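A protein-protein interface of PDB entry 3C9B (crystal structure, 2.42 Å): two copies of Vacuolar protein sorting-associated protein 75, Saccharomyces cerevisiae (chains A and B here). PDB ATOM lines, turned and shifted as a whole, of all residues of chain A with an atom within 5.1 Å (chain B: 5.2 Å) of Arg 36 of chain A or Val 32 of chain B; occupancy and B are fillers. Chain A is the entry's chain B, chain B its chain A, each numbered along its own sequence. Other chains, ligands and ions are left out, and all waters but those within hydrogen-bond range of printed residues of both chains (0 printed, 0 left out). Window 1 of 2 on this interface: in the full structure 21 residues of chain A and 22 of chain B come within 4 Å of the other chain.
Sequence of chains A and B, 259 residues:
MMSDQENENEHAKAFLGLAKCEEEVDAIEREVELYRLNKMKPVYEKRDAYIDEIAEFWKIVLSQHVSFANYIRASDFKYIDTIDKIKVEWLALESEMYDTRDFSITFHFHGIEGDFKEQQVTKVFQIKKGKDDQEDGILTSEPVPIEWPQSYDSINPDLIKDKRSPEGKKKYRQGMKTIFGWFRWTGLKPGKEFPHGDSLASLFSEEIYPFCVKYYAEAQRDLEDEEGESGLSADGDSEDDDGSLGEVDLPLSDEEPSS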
ATOM      1  N   VAL A  32     -19.929 -22.169   2.207  1.00  0.00           N
ATOM      2  CA  VAL A  32     -19.173 -22.801   1.134  1.00  0.00           C
ATOM      3  C   VAL A  32     -18.010 -23.669   1.653  1.00  0.00           C
ATOM      4  O   VAL A  32     -17.745 -24.731   1.086  1.00  0.00           O
ATOM      5  CB  VAL A  32     -18.556 -21.755   0.189  1.00  0.00           C
ATOM      6  CG1 VAL A  32     -19.647 -20.950  -0.501  1.00  0.00           C
ATOM      7  CG2 VAL A  32     -17.611 -20.840   0.950  1.00  0.00           C
ATOM      8  N   GLU A  33     -17.335 -23.240   2.726  1.00  0.00           N
ATOM      9  CA  GLU A  33     -16.284 -24.080   3.352  1.00  0.00           C
ATOM     10  C   GLU A  33     -16.889 -25.419   3.820  1.00  0.00           C
ATOM     11  O   GLU A  33     -16.293 -26.487   3.640  1.00  0.00           O
ATOM     12  CB  GLU A  33     -15.610 -23.367   4.542  1.00  0.00           C
ATOM     13  CG  GLU A  33     -14.973 -21.998   4.219  1.00  0.00           C
ATOM     14  CD  GLU A  33     -13.498 -22.077   3.769  1.00  0.00           C
ATOM     15  OE1 GLU A  33     -12.889 -23.183   3.855  1.00  0.00           O
ATOM     16  OE2 GLU A  33     -12.947 -21.016   3.342  1.00  0.00           O
ATOM     17  N   LEU A  34     -18.093 -25.328   4.382  1.00  0.00           N
ATOM     18  CA  LEU A  34     -18.871 -26.469   4.844  1.00  0.00           C
ATOM     19  C   LEU A  34     -19.341 -27.324   3.669  1.00  0.00           C
ATOM     20  O   LEU A  34     -19.371 -28.541   3.752  1.00  0.00           O
ATOM     21  CB  LEU A  34     -20.080 -25.958   5.633  1.00  0.00           C
ATOM     22  CG  LEU A  34     -20.378 -26.505   7.029  1.00  0.00           C
ATOM     23  CD1 LEU A  34     -19.116 -27.013   7.762  1.00  0.00           C
ATOM     24  CD2 LEU A  34     -21.094 -25.449   7.852  1.00  0.00           C
ATOM     25  N   TYR A  35     -19.709 -26.662   2.579  1.00  0.00           N
ATOM     26  CA  TYR A  35     -20.127 -27.325   1.353  1.00  0.00           C
ATOM     27  C   TYR A  35     -18.994 -28.186   0.813  1.00  0.00           C
ATOM     28  O   TYR A  35     -19.205 -29.329   0.442  1.00  0.00           O
ATOM     29  CB  TYR A  35     -20.556 -26.268   0.311  1.00  0.00           C
ATOM     30  CG  TYR A  35     -21.124 -26.828  -0.972  1.00  0.00           C
ATOM     31  CD1 TYR A  35     -22.410 -27.380  -1.011  1.00  0.00           C
ATOM     32  CD2 TYR A  35     -20.382 -26.798  -2.154  1.00  0.00           C
ATOM     33  CE1 TYR A  35     -22.940 -27.898  -2.198  1.00  0.00           C
ATOM     34  CE2 TYR A  35     -20.896 -27.316  -3.343  1.00  0.00           C
ATOM     35  CZ  TYR A  35     -22.175 -27.862  -3.358  1.00  0.00           C
ATOM     36  OH  TYR A  35     -22.688 -28.365  -4.533  1.00  0.00           O
ATOM     37  N   ARG A  36     -17.789 -27.617   0.795  1.00  0.00           N
ATOM     38  CA  ARG A  36     -16.590 -28.313   0.351  1.00  0.00           C
ATOM     39  C   ARG A  36     -16.285 -29.530   1.236  1.00  0.00           C
ATOM     40  O   ARG A  36     -16.043 -30.624   0.725  1.00  0.00           O
ATOM     41  CB  ARG A  36     -15.395 -27.356   0.328  1.00  0.00           C
ATOM     42  CG  ARG A  36     -14.117 -27.971  -0.234  1.00  0.00           C
ATOM     43  CD  ARG A  36     -12.861 -27.234   0.225  1.00  0.00           C
ATOM     44  NE  ARG A  36     -12.591 -26.059  -0.597  1.00  0.00           N
ATOM     45  CZ  ARG A  36     -12.698 -24.792  -0.182  1.00  0.00           C
ATOM     46  NH1 ARG A  36     -13.060 -24.511   1.074  1.00  0.00           N
ATOM     47  NH2 ARG A  36     -12.433 -23.792  -1.025  1.00  0.00           N
ATOM     48  N   LEU A  37     -16.320 -29.331   2.556  1.00  0.00           N
ATOM     49  CA  LEU A  37     -15.997 -30.390   3.519  1.00  0.00           C
ATOM     50  C   LEU A  37     -16.921 -31.591   3.389  1.00  0.00           C
ATOM     51  O   LEU A  37     -16.469 -32.735   3.382  1.00  0.00           O
ATOM     52  CB  LEU A  37     -16.015 -29.854   4.967  1.00  0.00           C
ATOM     53  CG  LEU A  37     -14.894 -28.885   5.391  1.00  0.00           C
ATOM     54  CD1 LEU A  37     -15.099 -28.331   6.820  1.00  0.00           C
ATOM     55  CD2 LEU A  37     -13.537 -29.541   5.244  1.00  0.00           C
ATOM     56  N   ASN A  38     -18.214 -31.325   3.289  1.00  0.00           N
ATOM     57  CA  ASN A  38     -19.196 -32.378   3.100  1.00  0.00           C
ATOM     58  C   ASN A  38     -19.022 -33.155   1.803  1.00  0.00           C
ATOM     59  O   ASN A  38     -19.279 -34.355   1.752  1.00  0.00           O
ATOM     60  CB  ASN A  38     -20.612 -31.806   3.189  1.00  0.00           C
ATOM     61  CG  ASN A  38     -21.090 -31.699   4.609  1.00  0.00           C
ATOM     62  OD1 ASN A  38     -21.044 -32.669   5.356  1.00  0.00           O
ATOM     63  ND2 ASN A  38     -21.529 -30.514   4.999  1.00  0.00           N
ATOM     64  N   LYS A  39     -18.586 -32.465   0.754  1.00  0.00           N
ATOM     65  CA  LYS A  39     -18.378 -33.092  -0.536  1.00  0.00           C
ATOM     66  C   LYS A  39     -17.076 -33.896  -0.570  1.00  0.00           C
ATOM     67  O   LYS A  39     -17.012 -34.954  -1.200  1.00  0.00           O
ATOM     68  CB  LYS A  39     -18.403 -32.039  -1.637  1.00  0.00           C
ATOM     69  CG  LYS A  39     -19.756 -31.331  -1.772  1.00  0.00           C
ATOM     70  CD  LYS A  39     -20.614 -31.951  -2.839  1.00  0.00           C
ATOM     71  CE  LYS A  39     -20.275 -31.360  -4.192  1.00  0.00           C
ATOM     72  NZ  LYS A  39     -20.751 -32.226  -5.302  1.00  0.00           N
ATOM     73  N   MET A  40     -16.051 -33.395   0.120  1.00  0.00           N
ATOM     74  CA  MET A  40     -14.731 -34.020   0.122  1.00  0.00           C
ATOM     75  C   MET A  40     -14.672 -35.271   0.997  1.00  0.00           C
ATOM     76  O   MET A  40     -13.812 -36.131   0.809  1.00  0.00           O
ATOM     77  CB  MET A  40     -13.678 -33.017   0.589  1.00  0.00           C
ATOM     78  CG  MET A  40     -13.424 -31.888  -0.393  1.00  0.00           C
ATOM     79  SD  MET A  40     -12.542 -32.518  -2.020  1.00  0.00           S
ATOM     80  CE  MET A  40     -10.684 -32.521  -1.366  1.00  0.00           C
ATOM     81  N   LYS A  41     -15.592 -35.353   1.951  1.00  0.00           N
ATOM     82  CA  LYS A  41     -15.586 -36.386   2.974  1.00  0.00           C
ATOM     83  C   LYS A  41     -15.669 -37.807   2.386  1.00  0.00           C
ATOM     84  O   LYS A  41     -14.794 -38.638   2.662  1.00  0.00           O
ATOM     85  CB  LYS A  41     -16.718 -36.139   3.968  1.00  0.00           C
ATOM     86  CG  LYS A  41     -16.567 -36.843   5.280  1.00  0.00           C
ATOM     87  CD  LYS A  41     -17.823 -36.669   6.118  1.00  0.00           C
ATOM     88  CE  LYS A  41     -17.694 -37.378   7.460  1.00  0.00           C
ATOM     89  NZ  LYS A  41     -17.540 -38.844   7.266  1.00  0.00           N
ATOM     90  N   ILE B  28     -14.891 -31.346  -7.808  1.00  0.00           N
ATOM     91  CA  ILE B  28     -15.485 -30.789  -6.590  1.00  0.00           C
ATOM     92  C   ILE B  28     -15.017 -29.361  -6.301  1.00  0.00           C
ATOM     93  O   ILE B  28     -15.821 -28.525  -5.921  1.00  0.00           O
ATOM     94  CB  ILE B  28     -15.253 -31.714  -5.353  1.00  0.00           C
ATOM     95  CG1 ILE B  28     -16.215 -32.900  -5.401  1.00  0.00           C
ATOM     96  CG2 ILE B  28     -15.432 -30.946  -4.032  1.00  0.00           C
ATOM     97  CD1 ILE B  28     -15.886 -34.009  -4.410  1.00  0.00           C
ATOM     98  N   GLU B  29     -13.728 -29.090  -6.496  1.00  0.00           N
ATOM     99  CA  GLU B  29     -13.181 -27.770  -6.197  1.00  0.00           C
ATOM    100  C   GLU B  29     -13.728 -26.678  -7.113  1.00  0.00           C
ATOM    101  O   GLU B  29     -13.877 -25.535  -6.683  1.00  0.00           O
ATOM    102  CB  GLU B  29     -11.646 -27.772  -6.213  1.00  0.00           C
ATOM    103  CG  GLU B  29     -10.984 -28.636  -5.099  1.00  0.00           C
ATOM    104  CD  GLU B  29     -11.027 -28.007  -3.681  1.00  0.00           C
ATOM    105  OE1 GLU B  29     -11.777 -27.022  -3.445  1.00  0.00           O
ATOM    106  OE2 GLU B  29     -10.304 -28.526  -2.796  1.00  0.00           O
ATOM    107  N   ARG B  30     -14.032 -27.019  -8.367  1.00  0.00           N
ATOM    108  CA  ARG B  30     -14.651 -26.048  -9.254  1.00  0.00           C
ATOM    109  C   ARG B  30     -16.126 -25.862  -8.921  1.00  0.00           C
ATOM    110  O   ARG B  30     -16.665 -24.757  -9.030  1.00  0.00           O
ATOM    111  CB  ARG B  30     -14.476 -26.416 -10.723  1.00  0.00           C
ATOM    112  CG  ARG B  30     -14.803 -25.237 -11.648  1.00  0.00           C
ATOM    113  CD  ARG B  30     -15.232 -25.686 -13.019  1.00  0.00           C
ATOM    114  NE  ARG B  30     -16.127 -24.711 -13.649  1.00  0.00           N
ATOM    115  CZ  ARG B  30     -15.725 -23.636 -14.329  1.00  0.00           C
ATOM    116  NH1 ARG B  30     -14.433 -23.370 -14.480  1.00  0.00           N
ATOM    117  NH2 ARG B  30     -16.625 -22.823 -14.854  1.00  0.00           N
ATOM    118  N   GLU B  31     -16.760 -26.953  -8.507  1.00  0.00           N
ATOM    119  CA  GLU B  31     -18.144 -26.960  -8.071  1.00  0.00           C
ATOM    120  C   GLU B  31     -18.360 -26.005  -6.891  1.00  0.00           C
ATOM    121  O   GLU B  31     -19.341 -25.264  -6.870  1.00  0.00           O
ATOM    122  CB  GLU B  31     -18.532 -28.377  -7.675  1.00  0.00           C
ATOM    123  CG  GLU B  31     -19.723 -28.955  -8.396  1.00  0.00           C
ATOM    124  CD  GLU B  31     -20.019 -30.402  -7.947  1.00  0.00           C
ATOM    125  OE1 GLU B  31     -19.315 -31.346  -8.401  1.00  0.00           O
ATOM    126  OE2 GLU B  31     -20.956 -30.584  -7.128  1.00  0.00           O
ATOM    127  N   VAL B  32     -17.436 -26.015  -5.922  1.00  0.00           N
ATOM    128  CA  VAL B  32     -17.538 -25.129  -4.748  1.00  0.00           C
ATOM    129  C   VAL B  32     -17.178 -23.683  -5.054  1.00  0.00           C
ATOM    130  O   VAL B  32     -17.750 -22.767  -4.467  1.00  0.00           O
ATOM    131  CB  VAL B  32     -16.598 -25.582  -3.616  1.00  0.00           C
ATOM    132  CG1 VAL B  32     -16.991 -26.965  -3.118  1.00  0.00           C
ATOM    133  CG2 VAL B  32     -15.153 -25.569  -4.088  1.00  0.00           C
ATOM    134  N   GLU B  33     -16.252 -23.485  -5.989  1.00  0.00           N
ATOM    135  CA  GLU B  33     -15.932 -22.151  -6.503  1.00  0.00           C
ATOM    136  C   GLU B  33     -17.142 -21.490  -7.179  1.00  0.00           C
ATOM    137  O   GLU B  33     -17.462 -20.337  -6.901  1.00  0.00           O
ATOM    138  CB  GLU B  33     -14.737 -22.222  -7.452  1.00  0.00           C
ATOM    139  CG  GLU B  33     -13.388 -22.284  -6.717  1.00  0.00           C
ATOM    140  CD  GLU B  33     -12.242 -22.856  -7.568  1.00  0.00           C
ATOM    141  OE1 GLU B  33     -12.432 -23.105  -8.793  1.00  0.00           O
ATOM    142  OE2 GLU B  33     -11.137 -23.060  -6.993  1.00  0.00           O
ATOM    143  N   LEU B  34     -17.826 -22.250  -8.034  1.00  0.00           N
ATOM    144  CA  LEU B  34     -19.078 -21.813  -8.662  1.00  0.00           C
ATOM    145  C   LEU B  34     -20.184 -21.564  -7.663  1.00  0.00           C
ATOM    146  O   LEU B  34     -20.986 -20.630  -7.823  1.00  0.00           O
ATOM    147  CB  LEU B  34     -19.548 -22.849  -9.669  1.00  0.00           C
ATOM    148  CG  LEU B  34     -19.053 -22.636 -11.089  1.00  0.00           C
ATOM    149  CD1 LEU B  34     -18.859 -23.966 -11.753  1.00  0.00           C
ATOM    150  CD2 LEU B  34     -20.051 -21.777 -11.868  1.00  0.00           C
ATOM    151  N   TYR B  35     -20.230 -22.418  -6.640  1.00  0.00           N
ATOM    152  CA  TYR B  35     -21.189 -22.308  -5.563  1.00  0.00           C
ATOM    153  C   TYR B  35     -20.998 -21.001  -4.790  1.00  0.00           C
ATOM    154  O   TYR B  35     -21.974 -20.328  -4.465  1.00  0.00           O
ATOM    155  CB  TYR B  35     -21.050 -23.512  -4.634  1.00  0.00           C
ATOM    156  CG  TYR B  35     -22.013 -23.545  -3.464  1.00  0.00           C
ATOM    157  CD1 TYR B  35     -23.245 -24.185  -3.572  1.00  0.00           C
ATOM    158  CD2 TYR B  35     -21.674 -22.963  -2.238  1.00  0.00           C
ATOM    159  CE1 TYR B  35     -24.134 -24.239  -2.491  1.00  0.00           C
ATOM    160  CE2 TYR B  35     -22.553 -23.000  -1.154  1.00  0.00           C
ATOM    161  CZ  TYR B  35     -23.783 -23.643  -1.288  1.00  0.00           C
ATOM    162  OH  TYR B  35     -24.663 -23.691  -0.217  1.00  0.00           O
ATOM    163  N   ARG B  36     -19.743 -20.654  -4.495  1.00  0.00           N
ATOM    164  CA  ARG B  36     -19.428 -19.404  -3.826  1.00  0.00           C
ATOM    165  C   ARG B  36     -19.803 -18.201  -4.708  1.00  0.00           C
ATOM    166  O   ARG B  36     -20.400 -17.240  -4.228  1.00  0.00           O
ATOM    167  CB  ARG B  36     -17.941 -19.340  -3.412  1.00  0.00           C
ATOM    168  CG  ARG B  36     -17.566 -18.000  -2.687  1.00  0.00           C
ATOM    169  CD  ARG B  36     -16.096 -17.893  -2.230  1.00  0.00           C
ATOM    170  NE  ARG B  36     -15.196 -18.555  -3.162  1.00  0.00           N
ATOM    171  CZ  ARG B  36     -14.331 -19.511  -2.823  1.00  0.00           C
ATOM    172  NH1 ARG B  36     -14.221 -19.889  -1.549  1.00  0.00           N
ATOM    173  NH2 ARG B  36     -13.561 -20.081  -3.759  1.00  0.00           N
ATOM    174  N   LEU B  37     -19.448 -18.267  -5.997  1.00  0.00           N
ATOM    175  CA  LEU B  37     -19.746 -17.176  -6.937  1.00  0.00           C
ATOM    176  C   LEU B  37     -21.260 -16.939  -7.107  1.00  0.00           C
ATOM    177  O   LEU B  37     -21.704 -15.806  -7.129  1.00  0.00           O
ATOM    178  CB  LEU B  37     -19.094 -17.429  -8.307  1.00  0.00           C
ATOM    179  CG  LEU B  37     -17.577 -17.477  -8.454  1.00  0.00           C
ATOM    180  CD1 LEU B  37     -17.246 -17.748  -9.912  1.00  0.00           C
ATOM    181  CD2 LEU B  37     -16.930 -16.196  -7.991  1.00  0.00           C
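NE of Arg 36 of chain A lies within salt-bridge range of OE1 of Glu 29 of chain B (3.1 Å).
The side-chain carboxylate of Glu 31 of chain B is in salt-bridge range of the side-chain amino group of Lys 39 of chain A.
The guanidinium group (NH1) of Arg 36 of chain A is in salt-bridge range of the side-chain carboxylate (OE1) of Glu 33 of chain A, at 3.1 Å.
CG1 of Val 32 of chain A touches CD2 of Tyr 35 of chain B, at 3.3 Å.
CG1 of Val 32 of chain A touches CA of Arg 36 of chain B, 3.7 Å away.
Tyr 35 of chain A touches Glu 31 of chain B.
Val 32 of chain B touches Tyr 35 of chain A (CG1 to CD2, 3.5 Å).
CZ of Tyr 35 of chain A touches CD1 of Tyr 35 of chain B, 3.8 Å away.
CG1 of Val 32 of chain B touches CA of Arg 36 of chain A, at 3.7 Å.
Ile 28 of chain B touches Lys 39 of chain A.
CG2 of Ile 28 of chain B touches SD of Met 40 of chain A, at 3.9 Å.
Of the printed residues of chain B, Val 32 of chain A touches Tyr 35 (3.3 Å) and Arg 36 (3.7 Å).
Arg 36 of chain A touches just these residues of chain B: Glu 29 (3.1 Å) and Val 32 (3.7 Å).
Printed residues of chain A within 4 Å of Glu 29 of chain B: Arg 36.
Of chain A, only Tyr 35 (3.5 Å) and Arg 36 (3.7 Å) come within 4 Å of Val 32 of chain B.
Of the printed residues of chain A, Arg 36 of chain B touches Val 32 (3.7 Å).
The nearest residue of chain B that does not touch Arg 36 of chain A is Arg 36 of chain B (4.3 Å).
Hydrophobic or aromatic side chains of chain A within 4 Å of the printed part of chain B: Val 32, Tyr 35 and Met 40.
Among the printed residues, 10 pairs touch across the chains.
Among the printed residues, Asp or Glu carboxylates within 4 Å of a Lys or Arg side-chain nitrogen of the other chain: Arg 36 of chain A with Glu 29 of chain B and Lys 39 of chain A with Glu 31 of chain B.
Val 32 of chain A touches Tyr 35 of chain B, and with the chains exchanged Tyr 35 of chain A touches Val 32 of chain B.
Val 32 of chain A touches Arg 36 of chain B, and with the chains exchanged Arg 36 of chain A touches Val 32 of chain B.
Tyr 35 of chain A touches its own counterpart, Tyr 35 of chain B.
Of the 10 pairs that touch across the chains among the printed residues, 5 have their exchanged pair printed and touching as well.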
